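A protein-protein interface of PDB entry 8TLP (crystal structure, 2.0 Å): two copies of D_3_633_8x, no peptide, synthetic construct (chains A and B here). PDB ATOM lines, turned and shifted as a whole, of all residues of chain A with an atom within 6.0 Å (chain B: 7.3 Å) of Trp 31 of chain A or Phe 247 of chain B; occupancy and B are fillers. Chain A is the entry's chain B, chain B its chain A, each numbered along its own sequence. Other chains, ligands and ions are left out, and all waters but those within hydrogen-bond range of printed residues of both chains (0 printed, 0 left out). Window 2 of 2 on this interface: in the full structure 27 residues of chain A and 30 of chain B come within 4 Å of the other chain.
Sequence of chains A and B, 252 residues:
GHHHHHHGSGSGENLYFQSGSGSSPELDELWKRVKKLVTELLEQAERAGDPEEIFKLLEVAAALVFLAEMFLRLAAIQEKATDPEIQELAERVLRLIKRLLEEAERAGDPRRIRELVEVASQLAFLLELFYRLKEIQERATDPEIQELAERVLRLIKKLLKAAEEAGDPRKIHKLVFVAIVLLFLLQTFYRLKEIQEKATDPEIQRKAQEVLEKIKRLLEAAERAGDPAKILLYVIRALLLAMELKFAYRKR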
ATOM      1  N   GLU A  26      26.881  21.337   6.885  1.00  0.00           N
ATOM      2  CA  GLU A  26      27.007  22.185   5.702  1.00  0.00           C
ATOM      3  C   GLU A  26      27.308  21.343   4.462  1.00  0.00           C
ATOM      4  O   GLU A  26      26.727  21.557   3.401  1.00  0.00           O
ATOM      5  CB  GLU A  26      28.094  23.247   5.902  1.00  0.00           C
ATOM      6  CG  GLU A  26      28.156  24.297   4.798  1.00  0.00           C
ATOM      7  N   LEU A  27      28.224  20.382   4.605  1.00  0.00           N
ATOM      8  CA  LEU A  27      28.508  19.466   3.508  1.00  0.00           C
ATOM      9  C   LEU A  27      27.267  18.665   3.128  1.00  0.00           C
ATOM     10  O   LEU A  27      27.013  18.417   1.938  1.00  0.00           O
ATOM     11  CB  LEU A  27      29.653  18.532   3.890  1.00  0.00           C
ATOM     12  CG  LEU A  27      31.020  18.811   3.261  1.00  0.00           C
ATOM     13  CD1 LEU A  27      31.859  17.530   3.225  1.00  0.00           C
ATOM     14  CD2 LEU A  27      30.896  19.411   1.872  1.00  0.00           C
ATOM     15  N   ASP A  28      26.470  18.266   4.124  1.00  0.00           N
ATOM     16  CA  ASP A  28      25.269  17.504   3.827  1.00  0.00           C
ATOM     17  C   ASP A  28      24.261  18.347   3.059  1.00  0.00           C
ATOM     18  O   ASP A  28      23.530  17.813   2.219  1.00  0.00           O
ATOM     19  CB  ASP A  28      24.662  16.951   5.118  1.00  0.00           C
ATOM     20  CG  ASP A  28      25.549  15.911   5.784  1.00  0.00           C
ATOM     21  N   GLU A  29      24.225  19.661   3.306  1.00  0.00           N
ATOM     22  CA  GLU A  29      23.329  20.537   2.561  1.00  0.00           C
ATOM     23  C   GLU A  29      23.843  20.820   1.157  1.00  0.00           C
ATOM     24  O   GLU A  29      23.040  20.975   0.230  1.00  0.00           O
ATOM     25  CB  GLU A  29      23.124  21.860   3.304  1.00  0.00           C
ATOM     26  N   LEU A  30      25.164  20.909   0.981  1.00  0.00           N
ATOM     27  CA  LEU A  30      25.702  21.075  -0.366  1.00  0.00           C
ATOM     28  C   LEU A  30      25.389  19.853  -1.225  1.00  0.00           C
ATOM     29  O   LEU A  30      24.945  19.997  -2.369  1.00  0.00           O
ATOM     30  CB  LEU A  30      27.211  21.334  -0.315  1.00  0.00           C
ATOM     31  CG  LEU A  30      27.681  22.791  -0.460  1.00  0.00           C
ATOM     32  N   TRP A  31      25.574  18.646  -0.674  1.00  0.00           N
ATOM     33  CA  TRP A  31      25.293  17.433  -1.433  1.00  0.00           C
ATOM     34  C   TRP A  31      23.825  17.353  -1.819  1.00  0.00           C
ATOM     35  O   TRP A  31      23.493  16.925  -2.934  1.00  0.00           O
ATOM     36  CB  TRP A  31      25.711  16.206  -0.627  1.00  0.00           C
ATOM     37  CG  TRP A  31      25.217  14.878  -1.153  1.00  0.00           C
ATOM     38  CD1 TRP A  31      24.607  13.902  -0.432  1.00  0.00           C
ATOM     39  CD2 TRP A  31      25.325  14.373  -2.496  1.00  0.00           C
ATOM     40  NE1 TRP A  31      24.322  12.823  -1.233  1.00  0.00           N
ATOM     41  CE2 TRP A  31      24.748  13.086  -2.506  1.00  0.00           C
ATOM     42  CE3 TRP A  31      25.855  14.880  -3.689  1.00  0.00           C
ATOM     43  CZ2 TRP A  31      24.681  12.301  -3.660  1.00  0.00           C
ATOM     44  CZ3 TRP A  31      25.782  14.098  -4.839  1.00  0.00           C
ATOM     45  CH2 TRP A  31      25.210  12.824  -4.814  1.00  0.00           C
ATOM     46  N   LYS A  32      22.933  17.790  -0.929  1.00  0.00           N
ATOM     47  CA  LYS A  32      21.516  17.785  -1.263  1.00  0.00           C
ATOM     48  C   LYS A  32      21.232  18.688  -2.451  1.00  0.00           C
ATOM     49  O   LYS A  32      20.440  18.331  -3.332  1.00  0.00           O
ATOM     50  CB  LYS A  32      20.686  18.211  -0.050  1.00  0.00           C
ATOM     51  N   ARG A  33      21.860  19.868  -2.491  1.00  0.00           N
ATOM     52  CA  ARG A  33      21.676  20.764  -3.630  1.00  0.00           C
ATOM     53  C   ARG A  33      22.295  20.188  -4.907  1.00  0.00           C
ATOM     54  O   ARG A  33      21.699  20.275  -5.992  1.00  0.00           O
ATOM     55  CB  ARG A  33      22.262  22.140  -3.308  1.00  0.00           C
ATOM     56  N   VAL A  34      23.499  19.615  -4.808  1.00  0.00           N
ATOM     57  CA  VAL A  34      24.100  18.968  -5.972  1.00  0.00           C
ATOM     58  C   VAL A  34      23.184  17.867  -6.484  1.00  0.00           C
ATOM     59  O   VAL A  34      22.859  17.811  -7.676  1.00  0.00           O
ATOM     60  CB  VAL A  34      25.499  18.422  -5.636  1.00  0.00           C
ATOM     61  CG1 VAL A  34      26.009  17.601  -6.789  1.00  0.00           C
ATOM     62  CG2 VAL A  34      26.459  19.560  -5.349  1.00  0.00           C
ATOM     63  N   LYS A  35      22.734  16.993  -5.580  1.00  0.00           N
ATOM     64  CA  LYS A  35      21.818  15.923  -5.971  1.00  0.00           C
ATOM     65  C   LYS A  35      20.607  16.481  -6.707  1.00  0.00           C
ATOM     66  O   LYS A  35      20.216  15.954  -7.754  1.00  0.00           O
ATOM     67  CB  LYS A  35      21.387  15.126  -4.735  1.00  0.00           C
ATOM     68  CG  LYS A  35      20.800  13.756  -5.030  1.00  0.00           C
ATOM     69  N   LYS A  36      20.026  17.575  -6.196  1.00  0.00           N
ATOM     70  CA  LYS A  36      18.857  18.177  -6.836  1.00  0.00           C
ATOM     71  C   LYS A  36      19.172  18.677  -8.242  1.00  0.00           C
ATOM     72  O   LYS A  36      18.386  18.452  -9.171  1.00  0.00           O
ATOM     73  CB  LYS A  36      18.315  19.328  -5.988  1.00  0.00           C
ATOM     74  N   LEU A  64      28.881  18.398 -11.959  1.00  0.00           N
ATOM     75  CA  LEU A  64      28.319  18.457 -10.612  1.00  0.00           C
ATOM     76  C   LEU A  64      28.741  17.252  -9.787  1.00  0.00           C
ATOM     77  O   LEU A  64      29.048  17.385  -8.598  1.00  0.00           O
ATOM     78  CB  LEU A  64      26.801  18.556 -10.673  1.00  0.00           C
ATOM     79  CG  LEU A  64      26.307  19.926 -11.127  1.00  0.00           C
ATOM     80  CD1 LEU A  64      24.827  19.875 -11.386  1.00  0.00           C
ATOM     81  CD2 LEU A  64      26.620  20.957 -10.059  1.00  0.00           C
ATOM     82  N   VAL A  65      28.781  16.067 -10.399  1.00  0.00           N
ATOM     83  CA  VAL A  65      29.224  14.898  -9.658  1.00  0.00           C
ATOM     84  C   VAL A  65      30.686  15.063  -9.260  1.00  0.00           C
ATOM     85  O   VAL A  65      31.069  14.770  -8.122  1.00  0.00           O
ATOM     86  CB  VAL A  65      28.983  13.611 -10.470  1.00  0.00           C
ATOM     87  CG1 VAL A  65      29.673  12.399  -9.771  1.00  0.00           C
ATOM     88  CG2 VAL A  65      27.482  13.351 -10.626  1.00  0.00           C
ATOM     89  N   ALA A  68      30.791  17.099  -6.077  1.00  0.00           N
ATOM     90  CA  ALA A  68      30.550  16.314  -4.872  1.00  0.00           C
ATOM     91  C   ALA A  68      31.783  15.506  -4.474  1.00  0.00           C
ATOM     92  O   ALA A  68      32.099  15.387  -3.286  1.00  0.00           O
ATOM     93  CB  ALA A  68      29.367  15.377  -5.081  1.00  0.00           C
ATOM     94  N   PHE A  71      34.131  17.633  -2.625  1.00  0.00           N
ATOM     95  CA  PHE A  71      33.651  17.804  -1.254  1.00  0.00           C
ATOM     96  C   PHE A  71      34.188  16.739  -0.311  1.00  0.00           C
ATOM     97  O   PHE A  71      34.379  16.999   0.882  1.00  0.00           O
ATOM     98  CB  PHE A  71      32.128  17.738  -1.226  1.00  0.00           C
ATOM     99  CG  PHE A  71      31.461  18.935  -1.806  1.00  0.00           C
ATOM    100  CD1 PHE A  71      30.101  18.915  -2.071  1.00  0.00           C
ATOM    101  CD2 PHE A  71      32.191  20.084  -2.079  1.00  0.00           C
ATOM    102  CE1 PHE A  71      29.483  20.010  -2.591  1.00  0.00           C
ATOM    103  CE2 PHE A  71      31.581  21.190  -2.598  1.00  0.00           C
ATOM    104  CZ  PHE A  71      30.221  21.164  -2.852  1.00  0.00           C
ATOM    105  N   LEU A  72      34.353  15.514  -0.800  1.00  0.00           N
ATOM    106  CA  LEU A  72      34.808  14.441   0.069  1.00  0.00           C
ATOM    107  C   LEU A  72      36.236  14.647   0.570  1.00  0.00           C
ATOM    108  O   LEU A  72      36.638  13.966   1.514  1.00  0.00           O
ATOM    109  CB  LEU A  72      34.702  13.106  -0.661  1.00  0.00           C
ATOM    110  CG  LEU A  72      33.300  12.618  -1.011  1.00  0.00           C
ATOM    111  CD1 LEU A  72      33.411  11.300  -1.740  1.00  0.00           C
ATOM    112  CD2 LEU A  72      32.436  12.473   0.248  1.00  0.00           C
ATOM    113  N   ILE B 195      35.258   0.098   0.641  1.00  0.00           N
ATOM    114  CA  ILE B 195      34.270   0.338   1.686  1.00  0.00           C
ATOM    115  C   ILE B 195      33.608  -0.967   2.087  1.00  0.00           C
ATOM    116  O   ILE B 195      33.429  -1.264   3.275  1.00  0.00           O
ATOM    117  CB  ILE B 195      33.220   1.360   1.211  1.00  0.00           C
ATOM    118  CG1 ILE B 195      33.821   2.761   1.068  1.00  0.00           C
ATOM    119  CG2 ILE B 195      32.006   1.359   2.148  1.00  0.00           C
ATOM    120  CD1 ILE B 195      32.833   3.786   0.513  1.00  0.00           C
ATOM    121  N   ILE B 204      25.910   0.458   6.208  1.00  0.00           N
ATOM    122  CA  ILE B 204      26.836   0.809   5.137  1.00  0.00           C
ATOM    123  C   ILE B 204      27.103  -0.398   4.252  1.00  0.00           C
ATOM    124  O   ILE B 204      27.109  -0.288   3.021  1.00  0.00           O
ATOM    125  CB  ILE B 204      28.140   1.391   5.707  1.00  0.00           C
ATOM    126  CG1 ILE B 204      27.858   2.754   6.303  1.00  0.00           C
ATOM    127  CG2 ILE B 204      29.161   1.588   4.590  1.00  0.00           C
ATOM    128  CD1 ILE B 204      27.445   3.765   5.246  1.00  0.00           C
ATOM    129  N   LEU B 239      27.414   7.009 -11.216  1.00  0.00           N
ATOM    130  CA  LEU B 239      28.240   7.874 -10.376  1.00  0.00           C
ATOM    131  C   LEU B 239      27.413   8.580  -9.313  1.00  0.00           C
ATOM    132  O   LEU B 239      27.855   8.718  -8.169  1.00  0.00           O
ATOM    133  CB  LEU B 239      28.950   8.904 -11.251  1.00  0.00           C
ATOM    134  CG  LEU B 239      30.118   8.323 -12.029  1.00  0.00           C
ATOM    135  CD1 LEU B 239      30.506   9.339 -13.040  1.00  0.00           C
ATOM    136  CD2 LEU B 239      31.278   8.062 -11.059  1.00  0.00           C
ATOM    137  N   LEU B 240      26.218   9.049  -9.681  1.00  0.00           N
ATOM    138  CA  LEU B 240      25.332   9.663  -8.693  1.00  0.00           C
ATOM    139  C   LEU B 240      24.973   8.664  -7.602  1.00  0.00           C
ATOM    140  O   LEU B 240      24.947   9.005  -6.409  1.00  0.00           O
ATOM    141  CB  LEU B 240      24.078  10.204  -9.395  1.00  0.00           C
ATOM    142  CG  LEU B 240      23.075  11.033  -8.573  1.00  0.00           C
ATOM    143  CD1 LEU B 240      23.698  12.346  -8.050  1.00  0.00           C
ATOM    144  CD2 LEU B 240      21.849  11.324  -9.403  1.00  0.00           C
ATOM    145  N   LEU B 241      24.742   7.409  -7.994  1.00  0.00           N
ATOM    146  CA  LEU B 241      24.423   6.365  -7.028  1.00  0.00           C
ATOM    147  C   LEU B 241      25.595   6.117  -6.100  1.00  0.00           C
ATOM    148  O   LEU B 241      25.427   6.075  -4.878  1.00  0.00           O
ATOM    149  CB  LEU B 241      24.054   5.065  -7.751  1.00  0.00           C
ATOM    150  CG  LEU B 241      22.610   4.834  -8.162  1.00  0.00           C
ATOM    151  CD1 LEU B 241      22.486   3.565  -8.995  1.00  0.00           C
ATOM    152  CD2 LEU B 241      21.723   4.767  -6.911  1.00  0.00           C
ATOM    153  N   ALA B 242      26.797   5.938  -6.668  1.00  0.00           N
ATOM    154  CA  ALA B 242      27.965   5.673  -5.837  1.00  0.00           C
ATOM    155  C   ALA B 242      28.253   6.838  -4.907  1.00  0.00           C
ATOM    156  O   ALA B 242      28.681   6.637  -3.765  1.00  0.00           O
ATOM    157  CB  ALA B 242      29.189   5.386  -6.704  1.00  0.00           C
ATOM    158  N   MET B 243      28.039   8.061  -5.386  1.00  0.00           N
ATOM    159  CA  MET B 243      28.289   9.237  -4.563  1.00  0.00           C
ATOM    160  C   MET B 243      27.343   9.303  -3.372  1.00  0.00           C
ATOM    161  O   MET B 243      27.720   9.797  -2.308  1.00  0.00           O
ATOM    162  CB  MET B 243      28.148  10.501  -5.405  1.00  0.00           C
ATOM    163  CG  MET B 243      28.666  11.765  -4.737  1.00  0.00           C
ATOM    164  SD  MET B 243      30.447  11.649  -4.432  1.00  0.00           S
ATOM    165  CE  MET B 243      31.059  11.358  -6.073  1.00  0.00           C
ATOM    166  N   GLU B 244      26.098   8.863  -3.545  1.00  0.00           N
ATOM    167  CA  GLU B 244      25.192   8.798  -2.406  1.00  0.00           C
ATOM    168  C   GLU B 244      25.774   7.914  -1.307  1.00  0.00           C
ATOM    169  O   GLU B 244      25.690   8.252  -0.118  1.00  0.00           O
ATOM    170  CB  GLU B 244      23.819   8.286  -2.853  1.00  0.00           C
ATOM    171  CG  GLU B 244      22.777   8.221  -1.736  1.00  0.00           C
ATOM    172  CD  GLU B 244      22.185   9.588  -1.414  1.00  0.00           C
ATOM    173  OE1 GLU B 244      21.955  10.382  -2.349  1.00  0.00           O
ATOM    174  OE2 GLU B 244      21.937   9.871  -0.226  1.00  0.00           O
ATOM    175  N   LEU B 245      26.403   6.797  -1.689  1.00  0.00           N
ATOM    176  CA  LEU B 245      27.013   5.909  -0.704  1.00  0.00           C
ATOM    177  C   LEU B 245      28.274   6.520  -0.100  1.00  0.00           C
ATOM    178  O   LEU B 245      28.498   6.410   1.111  1.00  0.00           O
ATOM    179  CB  LEU B 245      27.328   4.555  -1.344  1.00  0.00           C
ATOM    180  CG  LEU B 245      27.766   3.390  -0.443  1.00  0.00           C
ATOM    181  CD1 LEU B 245      29.281   3.362  -0.283  1.00  0.00           C
ATOM    182  CD2 LEU B 245      27.080   3.445   0.918  1.00  0.00           C
ATOM    183  N   LYS B 246      29.118   7.148  -0.927  1.00  0.00           N
ATOM    184  CA  LYS B 246      30.359   7.741  -0.428  1.00  0.00           C
ATOM    185  C   LYS B 246      30.082   8.868   0.563  1.00  0.00           C
ATOM    186  O   LYS B 246      30.777   8.992   1.574  1.00  0.00           O
ATOM    187  CB  LYS B 246      31.202   8.246  -1.596  1.00  0.00           C
ATOM    188  CG  LYS B 246      31.511   7.156  -2.619  1.00  0.00           C
ATOM    189  CD  LYS B 246      32.948   7.188  -3.079  1.00  0.00           C
ATOM    190  CE  LYS B 246      33.245   8.437  -3.876  1.00  0.00           C
ATOM    191  NZ  LYS B 246      34.687   8.809  -3.722  1.00  0.00           N
ATOM    192  N   PHE B 247      29.068   9.690   0.296  1.00  0.00           N
ATOM    193  CA  PHE B 247      28.704  10.740   1.239  1.00  0.00           C
ATOM    194  C   PHE B 247      28.172  10.153   2.546  1.00  0.00           C
ATOM    195  O   PHE B 247      28.447  10.684   3.631  1.00  0.00           O
ATOM    196  CB  PHE B 247      27.673  11.671   0.601  1.00  0.00           C
ATOM    197  CG  PHE B 247      28.277  12.882  -0.062  1.00  0.00           C
ATOM    198  CD1 PHE B 247      28.485  14.058   0.650  1.00  0.00           C
ATOM    199  CE1 PHE B 247      29.050  15.183   0.033  1.00  0.00           C
ATOM    200  N   ALA B 248      27.408   9.056   2.461  1.00  0.00           N
ATOM    201  CA  ALA B 248      26.938   8.374   3.663  1.00  0.00           C
ATOM    202  C   ALA B 248      28.097   7.823   4.487  1.00  0.00           C
ATOM    203  O   ALA B 248      28.055   7.863   5.721  1.00  0.00           O
ATOM    204  CB  ALA B 248      25.970   7.248   3.287  1.00  0.00           C
ATOM    205  N   TYR B 249      29.146   7.312   3.835  1.00  0.00           N
ATOM    206  CA  TYR B 249      30.239   6.714   4.596  1.00  0.00           C
ATOM    207  C   TYR B 249      31.123   7.769   5.258  1.00  0.00           C
ATOM    208  O   TYR B 249      31.657   7.530   6.350  1.00  0.00           O
ATOM    209  CB  TYR B 249      31.075   5.803   3.712  1.00  0.00           C
ATOM    210  CG  TYR B 249      31.913   4.845   4.510  1.00  0.00           C
ATOM    211  CD1 TYR B 249      33.206   4.552   4.124  1.00  0.00           C
ATOM    212  CD2 TYR B 249      31.414   4.236   5.655  1.00  0.00           C
ATOM    213  CE1 TYR B 249      33.982   3.678   4.840  1.00  0.00           C
ATOM    214  CE2 TYR B 249      32.190   3.346   6.386  1.00  0.00           C
ATOM    215  CZ  TYR B 249      33.477   3.073   5.963  1.00  0.00           C
ATOM    216  OH  TYR B 249      34.283   2.201   6.659  1.00  0.00           O
ATOM    217  N   ARG B 250      31.322   8.915   4.605  1.00  0.00           N
ATOM    218  CA  ARG B 250      31.875  10.114   5.261  1.00  0.00           C
ATOM    219  C   ARG B 250      31.818  11.321   4.332  1.00  0.00           C
ATOM    220  O   ARG B 250      30.914  12.153   4.438  1.00  0.00           O
ATOM    221  CB  ARG B 250      33.321   9.899   5.747  1.00  0.00           C
ATOM    222  CG  ARG B 250      33.465   9.986   7.264  1.00  0.00           C
ATOM    223  CD  ARG B 250      34.305  11.185   7.731  1.00  0.00           C
ATOM    224  NE  ARG B 250      33.756  12.470   7.293  1.00  0.00           N
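No position is printed for both chains.
Of the 16 printed residues of chain A, 4 touch a printed residue of chain B. Printed residues of chain A that touch a printed residue of chain B: Trp 31, Val 65, Ala 68 and Leu 72. Hydrophobic or aromatic side chains of chain A that line the printed part of chain B: Trp 31, Val 65, Ala 68 and Leu 72. Of the 14 printed residues of chain B, 6 touch a printed residue of chain A. Hydrophobic or aromatic side chains of chain B that line the printed part of chain A: Leu 239, Leu 240, Met 243 and Phe 247. Among the printed residues, 8 pairs touch across the chains.
Trp 31 of chain A touches just these residues of chain B: Leu 240, Met 243, Glu 244 and Phe 247. Of the printed residues of chain A, Phe 247 of chain B touches Trp 31 (3.6 Å). Of the printed residues of chain A, Glu 244 of chain B touches Trp 31. Of the printed residues of chain A, Met 243 of chain B touches Trp 31, Val 65 and Ala 68. Of the printed residues of chain A, Leu 240 of chain B touches Trp 31 (3.6 Å). Printed residues of chain A within 4 Å of Leu 239 of chain B: Val 65. Phe 71 of chain A touches none of the printed residues of chain B. Leu 241 of chain B touches none of the printed residues of chain A. The nearest printed residue of chain A that does not touch Phe 247 of chain B is Leu 72 of chain A (4.2 Å). The nearest printed residue of chain A that does not touch Lys 246 of chain B is Ala 68 of chain A (7.1 Å).
Among the printed residues, pairs that only touch across the chains: Trp 31 of chain A with Leu 240 of chain B (3.6 Å), Trp 31 of chain A with Met 243 of chain B (3.6 Å), Trp 31 of chain A with Glu 244 of chain B (3.6 Å), Trp 31 of chain A with Phe 247 of chain B (3.6 Å), Val 65 of chain A with Leu 239 of chain B (3.9 Å), Val 65 of chain A with Met 243 of chain B (3.98 Å), Ala 68 of chain A with Met 243 of chain B (3.7 Å) and Leu 72 of chain A with Lys 246 of chain B (3.4 Å).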
